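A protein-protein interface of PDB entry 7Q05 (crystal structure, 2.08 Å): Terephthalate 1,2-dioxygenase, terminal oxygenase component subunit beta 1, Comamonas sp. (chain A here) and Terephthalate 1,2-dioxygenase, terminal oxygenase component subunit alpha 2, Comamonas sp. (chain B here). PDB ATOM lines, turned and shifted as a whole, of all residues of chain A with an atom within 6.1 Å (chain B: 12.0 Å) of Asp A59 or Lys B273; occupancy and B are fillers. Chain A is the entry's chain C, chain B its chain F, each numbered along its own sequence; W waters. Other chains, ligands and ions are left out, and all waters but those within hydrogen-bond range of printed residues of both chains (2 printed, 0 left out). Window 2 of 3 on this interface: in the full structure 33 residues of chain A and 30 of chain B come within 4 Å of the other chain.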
ATOM      1  N   LYS A  32       0.828  -3.654  35.926  1.00  0.00           N
ATOM      2  CA  LYS A  32       1.060  -3.953  34.502  1.00  0.00           C
ATOM      3  C   LYS A  32       1.680  -2.743  33.808  1.00  0.00           C
ATOM      4  O   LYS A  32       2.617  -2.980  33.027  1.00  0.00           O
ATOM      5  CB  LYS A  32      -0.215  -4.397  33.774  1.00  0.00           C
ATOM      6  CG  LYS A  32      -0.281  -5.889  33.479  1.00  0.00           C
ATOM      7  CD  LYS A  32      -0.154  -6.764  34.714  1.00  0.00           C
ATOM      8  CE  LYS A  32      -0.415  -8.244  34.464  1.00  0.00           C
ATOM      9  NZ  LYS A  32       0.853  -9.002  34.271  1.00  0.00           N
ATOM     10  N   SER A  57       6.580  -0.794  31.803  1.00  0.00           N
ATOM     11  CA  SER A  57       5.631  -1.925  31.894  1.00  0.00           C
ATOM     12  C   SER A  57       6.208  -3.038  32.769  1.00  0.00           C
ATOM     13  O   SER A  57       7.442  -3.159  32.872  1.00  0.00           O
ATOM     14  CB  SER A  57       5.249  -2.445  30.540  1.00  0.00           C
ATOM     15  OG  SER A  57       6.219  -3.379  30.106  1.00  0.00           O
ATOM     16  N   GLN A  58       5.339  -3.867  33.334  1.00  0.00           N
ATOM     17  CA  GLN A  58       5.750  -5.040  34.133  1.00  0.00           C
ATOM     18  C   GLN A  58       6.470  -6.014  33.208  1.00  0.00           C
ATOM     19  O   GLN A  58       7.468  -6.613  33.625  1.00  0.00           O
ATOM     20  CB  GLN A  58       4.550  -5.701  34.804  1.00  0.00           C
ATOM     21  CG  GLN A  58       4.984  -6.747  35.822  1.00  0.00           C
ATOM     22  CD  GLN A  58       3.811  -7.579  36.265  1.00  0.00           C
ATOM     23  OE1 GLN A  58       3.358  -8.451  35.570  1.00  0.00           O
ATOM     24  NE2 GLN A  58       3.310  -7.301  37.447  1.00  0.00           N
ATOM     25  N   ASP A  59       6.011  -6.129  31.981  1.00  0.00           N
ATOM     26  CA  ASP A  59       6.639  -6.992  30.953  1.00  0.00           C
ATOM     27  C   ASP A  59       8.121  -6.602  30.761  1.00  0.00           C
ATOM     28  O   ASP A  59       8.956  -7.534  30.673  1.00  0.00           O
ATOM     29  CB  ASP A  59       5.792  -6.940  29.685  1.00  0.00           C
ATOM     30  CG  ASP A  59       4.554  -7.808  29.792  1.00  0.00           C
ATOM     31  OD1 ASP A  59       4.491  -8.601  30.710  1.00  0.00           O
ATOM     32  OD2 ASP A  59       3.677  -7.703  28.929  1.00  0.00           O
ATOM     33  N   MET A  60       8.465  -5.305  30.742  1.00  0.00           N
ATOM     34  CA  MET A  60       9.885  -4.876  30.618  1.00  0.00           C
ATOM     35  C   MET A  60      10.690  -5.394  31.807  1.00  0.00           C
ATOM     36  O   MET A  60      11.828  -5.848  31.591  1.00  0.00           O
ATOM     37  CB  MET A  60      10.029  -3.359  30.506  1.00  0.00           C
ATOM     38  CG  MET A  60       9.670  -2.846  29.131  1.00  0.00           C
ATOM     39  SD  MET A  60      10.087  -1.127  28.919  1.00  0.00           S
ATOM     40  CE  MET A  60      11.878  -1.161  28.934  1.00  0.00           C
ATOM     41  N   LEU A  61      10.107  -5.380  32.998  1.00  0.00           N
ATOM     42  CA  LEU A  61      10.775  -5.893  34.218  1.00  0.00           C
ATOM     43  C   LEU A  61      11.018  -7.398  34.061  1.00  0.00           C
ATOM     44  O   LEU A  61      12.158  -7.845  34.375  1.00  0.00           O
ATOM     45  CB  LEU A  61       9.925  -5.608  35.458  1.00  0.00           C
ATOM     46  CG  LEU A  61       9.519  -4.159  35.698  1.00  0.00           C
ATOM     47  CD1 LEU A  61       8.743  -4.060  36.994  1.00  0.00           C
ATOM     48  CD2 LEU A  61      10.728  -3.247  35.747  1.00  0.00           C
ATOM     49  N   THR A  62      10.018  -8.139  33.597  1.00  0.00           N
ATOM     50  CA  THR A  62      10.103  -9.611  33.390  1.00  0.00           C
ATOM     51  C   THR A  62      11.232  -9.918  32.397  1.00  0.00           C
ATOM     52  O   THR A  62      12.028 -10.813  32.677  1.00  0.00           O
ATOM     53  CB  THR A  62       8.737 -10.184  32.967  1.00  0.00           C
ATOM     54  OG1 THR A  62       7.790  -9.890  33.994  1.00  0.00           O
ATOM     55  CG2 THR A  62       8.754 -11.676  32.762  1.00  0.00           C
ATOM     56  N   ASP A  63      11.287  -9.200  31.271  1.00  0.00           N
ATOM     57  CA  ASP A  63      12.350  -9.373  30.241  1.00  0.00           C
ATOM     58  C   ASP A  63      13.717  -9.098  30.857  1.00  0.00           C
ATOM     59  O   ASP A  63      14.655  -9.822  30.550  1.00  0.00           O
ATOM     60  CB  ASP A  63      12.125  -8.468  29.036  1.00  0.00           C
ATOM     61  CG  ASP A  63      10.923  -8.896  28.230  1.00  0.00           C
ATOM     62  OD1 ASP A  63      10.569 -10.081  28.308  1.00  0.00           O
ATOM     63  OD2 ASP A  63      10.344  -8.039  27.540  1.00  0.00           O
ATOM     64  N   ARG A  64      13.847  -8.096  31.703  1.00  0.00           N
ATOM     65  CA  ARG A  64      15.163  -7.767  32.321  1.00  0.00           C
ATOM     66  C   ARG A  64      15.606  -8.960  33.176  1.00  0.00           C
ATOM     67  O   ARG A  64      16.815  -9.280  33.139  1.00  0.00           O
ATOM     68  CB  ARG A  64      15.119  -6.440  33.073  1.00  0.00           C
ATOM     69  CG  ARG A  64      16.376  -6.120  33.859  1.00  0.00           C
ATOM     70  CD  ARG A  64      16.460  -4.663  34.327  1.00  0.00           C
ATOM     71  NE  ARG A  64      16.881  -3.775  33.262  1.00  0.00           N
ATOM     72  CZ  ARG A  64      18.134  -3.592  32.850  1.00  0.00           C
ATOM     73  NH1 ARG A  64      19.122  -4.275  33.395  1.00  0.00           N
ATOM     74  NH2 ARG A  64      18.398  -2.738  31.862  1.00  0.00           N
ATOM     75  N   PHE B 219      23.263 -11.264  23.981  1.00  0.00           N
ATOM     76  CA  PHE B 219      21.870 -10.756  24.049  1.00  0.00           C
ATOM     77  C   PHE B 219      21.111 -11.076  22.746  1.00  0.00           C
ATOM     78  O   PHE B 219      20.029 -11.705  22.879  1.00  0.00           O
ATOM     79  CB  PHE B 219      21.794  -9.268  24.417  1.00  0.00           C
ATOM     80  CG  PHE B 219      20.379  -8.737  24.499  1.00  0.00           C
ATOM     81  CD1 PHE B 219      19.548  -9.089  25.564  1.00  0.00           C
ATOM     82  CD2 PHE B 219      19.855  -7.922  23.494  1.00  0.00           C
ATOM     83  CE1 PHE B 219      18.243  -8.615  25.639  1.00  0.00           C
ATOM     84  CE2 PHE B 219      18.549  -7.457  23.569  1.00  0.00           C
ATOM     85  CZ  PHE B 219      17.750  -7.799  24.643  1.00  0.00           C
ATOM     86  N   THR B 222      21.180 -15.182  22.178  1.00  0.00           N
ATOM     87  CA  THR B 222      20.289 -15.907  23.136  1.00  0.00           C
ATOM     88  C   THR B 222      18.824 -15.736  22.689  1.00  0.00           C
ATOM     89  O   THR B 222      18.084 -16.738  22.746  1.00  0.00           O
ATOM     90  CB  THR B 222      20.504 -15.492  24.605  1.00  0.00           C
ATOM     91  OG1 THR B 222      20.288 -14.085  24.759  1.00  0.00           O
ATOM     92  CG2 THR B 222      21.870 -15.889  25.129  1.00  0.00           C
ATOM     93  N   PHE B 223      18.423 -14.531  22.243  1.00  0.00           N
ATOM     94  CA  PHE B 223      17.012 -14.159  21.938  1.00  0.00           C
ATOM     95  C   PHE B 223      16.786 -14.106  20.407  1.00  0.00           C
ATOM     96  O   PHE B 223      17.032 -13.085  19.717  1.00  0.00           O
ATOM     97  CB  PHE B 223      16.627 -12.867  22.674  1.00  0.00           C
ATOM     98  CG  PHE B 223      16.551 -12.983  24.184  1.00  0.00           C
ATOM     99  CD1 PHE B 223      15.516 -13.683  24.796  1.00  0.00           C
ATOM    100  CD2 PHE B 223      17.502 -12.393  25.009  1.00  0.00           C
ATOM    101  CE1 PHE B 223      15.434 -13.786  26.182  1.00  0.00           C
ATOM    102  CE2 PHE B 223      17.426 -12.507  26.393  1.00  0.00           C
ATOM    103  CZ  PHE B 223      16.396 -13.205  26.977  1.00  0.00           C
ATOM    104  N   ARG B 271       9.989 -14.423  22.539  1.00  0.00           N
ATOM    105  CA  ARG B 271      11.288 -14.125  23.216  1.00  0.00           C
ATOM    106  C   ARG B 271      11.108 -12.958  24.214  1.00  0.00           C
ATOM    107  O   ARG B 271      11.066 -13.262  25.408  1.00  0.00           O
ATOM    108  CB  ARG B 271      12.382 -13.924  22.159  1.00  0.00           C
ATOM    109  CG  ARG B 271      12.765 -15.217  21.448  1.00  0.00           C
ATOM    110  CD  ARG B 271      13.747 -16.062  22.251  1.00  0.00           C
ATOM    111  NE  ARG B 271      13.201 -16.752  23.421  1.00  0.00           N
ATOM    112  CZ  ARG B 271      13.906 -17.151  24.484  1.00  0.00           C
ATOM    113  NH1 ARG B 271      13.310 -17.793  25.469  1.00  0.00           N
ATOM    114  NH2 ARG B 271      15.200 -16.912  24.583  1.00  0.00           N
ATOM    115  N   LEU B 272      11.023 -11.697  23.764  1.00  0.00           N
ATOM    116  CA  LEU B 272      10.721 -10.498  24.607  1.00  0.00           C
ATOM    117  C   LEU B 272       9.214 -10.388  24.831  1.00  0.00           C
ATOM    118  O   LEU B 272       8.511 -10.329  23.816  1.00  0.00           O
ATOM    119  CB  LEU B 272      11.163  -9.223  23.889  1.00  0.00           C
ATOM    120  CG  LEU B 272      12.659  -8.986  23.765  1.00  0.00           C
ATOM    121  CD1 LEU B 272      12.887  -7.680  23.025  1.00  0.00           C
ATOM    122  CD2 LEU B 272      13.353  -8.969  25.127  1.00  0.00           C
ATOM    123  N   LYS B 273       8.735 -10.255  26.075  1.00  0.00           N
ATOM    124  CA  LYS B 273       7.285 -10.015  26.353  1.00  0.00           C
ATOM    125  C   LYS B 273       6.915  -8.569  25.989  1.00  0.00           C
ATOM    126  O   LYS B 273       5.747  -8.316  25.775  1.00  0.00           O
ATOM    127  CB  LYS B 273       6.916 -10.261  27.821  1.00  0.00           C
ATOM    128  CG  LYS B 273       7.240 -11.629  28.394  1.00  0.00           C
ATOM    129  CD  LYS B 273       6.433 -11.951  29.632  1.00  0.00           C
ATOM    130  CE  LYS B 273       4.963 -12.175  29.329  1.00  0.00           C
ATOM    131  NZ  LYS B 273       4.106 -12.033  30.525  1.00  0.00           N
ATOM    132  N   ASP B 274       7.860  -7.633  26.004  1.00  0.00           N
ATOM    133  CA  ASP B 274       7.607  -6.242  25.536  1.00  0.00           C
ATOM    134  C   ASP B 274       8.656  -5.945  24.466  1.00  0.00           C
ATOM    135  O   ASP B 274       9.782  -5.525  24.747  1.00  0.00           O
ATOM    136  CB  ASP B 274       7.485  -5.247  26.711  1.00  0.00           C
ATOM    137  CG  ASP B 274       6.837  -3.852  26.331  1.00  0.00           C
ATOM    138  OD1 ASP B 274       7.136  -3.397  25.192  1.00  0.00           O
ATOM    139  OD2 ASP B 274       6.241  -3.232  27.194  1.00  0.00           O
ATOM    140  N   PRO B 275       8.319  -6.256  23.194  1.00  0.00           N
ATOM    141  CA  PRO B 275       9.196  -5.987  22.049  1.00  0.00           C
ATOM    142  C   PRO B 275       9.576  -4.503  21.918  1.00  0.00           C
ATOM    143  O   PRO B 275      10.548  -4.235  21.262  1.00  0.00           O
ATOM    144  CB  PRO B 275       8.375  -6.401  20.809  1.00  0.00           C
ATOM    145  CG  PRO B 275       7.281  -7.321  21.343  1.00  0.00           C
ATOM    146  CD  PRO B 275       7.058  -6.902  22.787  1.00  0.00           C
ATOM    147  N   SER B 276       8.819  -3.585  22.535  1.00  0.00           N
ATOM    148  CA  SER B 276       9.043  -2.109  22.445  1.00  0.00           C
ATOM    149  C   SER B 276      10.469  -1.706  22.874  1.00  0.00           C
ATOM    150  O   SER B 276      10.886  -0.589  22.561  1.00  0.00           O
ATOM    151  CB  SER B 276       7.969  -1.325  23.196  1.00  0.00           C
ATOM    152  OG  SER B 276       8.328  -1.083  24.560  1.00  0.00           O
ATOM    153  N   LEU B 277      11.200  -2.572  23.579  1.00  0.00           N
ATOM    154  CA  LEU B 277      12.608  -2.312  23.952  1.00  0.00           C
ATOM    155  C   LEU B 277      13.417  -2.009  22.687  1.00  0.00           C
ATOM    156  O   LEU B 277      14.327  -1.202  22.772  1.00  0.00           O
ATOM    157  CB  LEU B 277      13.172  -3.534  24.680  1.00  0.00           C
ATOM    158  CG  LEU B 277      14.678  -3.526  24.910  1.00  0.00           C
ATOM    159  CD1 LEU B 277      15.054  -2.394  25.819  1.00  0.00           C
ATOM    160  CD2 LEU B 277      15.131  -4.836  25.512  1.00  0.00           C
ATOM    161  N   LEU B 278      13.127  -2.684  21.573  1.00  0.00           N
ATOM    162  CA  LEU B 278      13.950  -2.655  20.340  1.00  0.00           C
ATOM    163  C   LEU B 278      13.195  -1.942  19.215  1.00  0.00           C
ATOM    164  O   LEU B 278      13.797  -1.768  18.160  1.00  0.00           O
ATOM    165  CB  LEU B 278      14.285  -4.097  19.944  1.00  0.00           C
ATOM    166  CG  LEU B 278      15.245  -4.811  20.893  1.00  0.00           C
ATOM    167  CD1 LEU B 278      15.516  -6.229  20.418  1.00  0.00           C
ATOM    168  CD2 LEU B 278      16.552  -4.027  21.053  1.00  0.00           C
ATOM    169  N   GLU B 279      11.935  -1.543  19.414  1.00  0.00           N
ATOM    170  CA  GLU B 279      11.196  -0.682  18.449  1.00  0.00           C
ATOM    171  C   GLU B 279      11.898   0.667  18.380  1.00  0.00           C
ATOM    172  O   GLU B 279      12.262   1.233  19.453  1.00  0.00           O
ATOM    173  CB  GLU B 279       9.719  -0.537  18.793  1.00  0.00           C
ATOM    174  CG  GLU B 279       8.939  -1.796  18.427  1.00  0.00           C
ATOM    175  CD  GLU B 279       7.551  -1.925  19.046  1.00  0.00           C
ATOM    176  OE1 GLU B 279       7.131  -0.981  19.784  1.00  0.00           O
ATOM    177  OE2 GLU B 279       6.899  -2.973  18.804  1.00  0.00           O
ATOM    178  N   LYS B 343      13.801   3.957  26.519  1.00  0.00           N
ATOM    179  CA  LYS B 343      13.674   2.484  26.543  1.00  0.00           C
ATOM    180  C   LYS B 343      14.934   1.805  26.014  1.00  0.00           C
ATOM    181  O   LYS B 343      15.385   0.839  26.631  1.00  0.00           O
ATOM    182  CB  LYS B 343      12.474   2.008  25.737  1.00  0.00           C
ATOM    183  CG  LYS B 343      11.137   2.402  26.327  1.00  0.00           C
ATOM    184  CD  LYS B 343       9.997   1.505  25.795  1.00  0.00           C
ATOM    185  CE  LYS B 343       8.725   2.277  25.549  1.00  0.00           C
ATOM    186  NZ  LYS B 343       7.565   1.376  25.423  1.00  0.00           N
ATOM    187  N   ASN B 346      18.259   0.905  27.977  1.00  0.00           N
ATOM    188  CA  ASN B 346      18.392  -0.355  28.756  1.00  0.00           C
ATOM    189  C   ASN B 346      19.506  -1.220  28.166  1.00  0.00           C
ATOM    190  O   ASN B 346      19.982  -2.117  28.906  1.00  0.00           O
ATOM    191  CB  ASN B 346      17.074  -1.109  28.859  1.00  0.00           C
ATOM    192  CG  ASN B 346      16.109  -0.419  29.812  1.00  0.00           C
ATOM    193  OD1 ASN B 346      16.275  -0.435  31.016  1.00  0.00           O
ATOM    194  ND2 ASN B 346      15.084   0.189  29.295  1.00  0.00           N
ATOM    195  N   PHE B 353      21.827  -4.450  28.805  1.00  0.00           N
ATOM    196  CA  PHE B 353      21.711  -5.806  28.210  1.00  0.00           C
ATOM    197  C   PHE B 353      22.964  -6.161  27.381  1.00  0.00           C
ATOM    198  O   PHE B 353      23.376  -7.358  27.338  1.00  0.00           O
ATOM    199  CB  PHE B 353      20.444  -5.896  27.365  1.00  0.00           C
ATOM    200  CG  PHE B 353      19.178  -5.703  28.165  1.00  0.00           C
ATOM    201  CD1 PHE B 353      19.024  -6.313  29.399  1.00  0.00           C
ATOM    202  CD2 PHE B 353      18.129  -4.950  27.664  1.00  0.00           C
ATOM    203  CE1 PHE B 353      17.861  -6.137  30.124  1.00  0.00           C
ATOM    204  CE2 PHE B 353      16.965  -4.779  28.397  1.00  0.00           C
ATOM    205  CZ  PHE B 353      16.851  -5.335  29.642  1.00  0.00           C
HETATM  206  O   HOH W   1      14.501  -2.828  31.660  1.00  0.00           O
HETATM  207  O   HOH W   2      11.650  -5.567  27.283  1.00  0.00           O
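OG of Ser A57 lies close to N of Asp A59, at 3.3 Å.
The backbone NH (N) of Met A60 lies within hydrogen-bond range of the side-chain hydroxyl (OG) of Ser A57 (3.0 Å).
O of Gln A58 is in hydrogen-bond range of OG1 of Thr A62 (3.3 Å).
OD1 of Asp B274 sits at hydrogen-bond distance from OG of Ser B276 (2.7 Å).
O of Lys B343 sits at hydrogen-bond distance from ND2 of Asn B346 (2.8 Å).
O of Asn B346 is in hydrogen-bond range of N of Phe B353, at 3.0 Å.
Water W2 bridges OD2 of Asp A63 and O of Asp B274.
Water W1 lies within hydrogen-bond range of the guanidinium group (NE) of Arg A64 (3.0 Å) and the side-chain amide oxygen (OD1) of Asn B346 (3.0 Å).
Of chain B, only Lys B273 and Asp B274 come within 4 Å of Asp A59.
Lys B273 touches three residues of chain A.
Of the printed residues of chain B, Ser A57 touches Asp B274 (2.9 Å).
No residue of chain B comes within 4 Å of Gln A58.
No residue of chain B comes within 4 Å of Leu A61.
Thr A62 touches just one residue of chain B: Lys B273 (3.9 Å).
Of the printed residues of chain A, Asp B274 touches Ser A57 (2.9 Å), Asp A59 (3.8 Å), Met A60 (3.96 Å) and Asp A63 (2.9 Å).
Printed residues of chain A within 4 Å of Asn B346: Met A60 (3.5 Å) and Arg A64 (3.2 Å).
The nearest residue of chain A that does not touch Lys B273 is Lys A32 (5.8 Å).
The nearest printed residue of chain A that does not touch Leu B272 is Asp A59 (6.5 Å).
Of the 15 printed residues of chain B, 5 touch a printed residue of chain A.
Hydrophobic or aromatic side chains of chain B within 4 Å of the printed part of chain A: Leu B272 and Phe B353.
Of the 9 printed residues of chain A, 6 touch a printed residue of chain B.
Among the printed residues, 11 pairs touch across the chains.
Among the printed residues, pairs that only touch across the chains: Met A60 with Asn B346 (3.5 Å), Asp A63 with Leu B272 (3.7 Å), Arg A64 with Phe B353 (3.7 Å), Asp A59 with Asp B274 (3.8 Å), Thr A62 with Lys B273 (3.9 Å) and Met A60 with Asp B274 (3.96 Å).
OD2 of Asp B274 lies within hydrogen-bond range of OG of Ser A57, 2.9 Å away.
The side-chain carboxylate (OD1) of Asp A59 is in salt-bridge range of the side-chain amino group (NZ) of Lys B273 (3.5 Å).
OD1 of Asp A63 lies within hydrogen-bond range of N of Lys B273.
N of Asp B274 is in hydrogen-bond range of OD2 of Asp A63, 2.9 Å away.
The guanidinium group (NH2) of Arg A64 is in hydrogen-bond range of the side-chain amide oxygen (OD1) of Asn B346 (3.2 Å).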
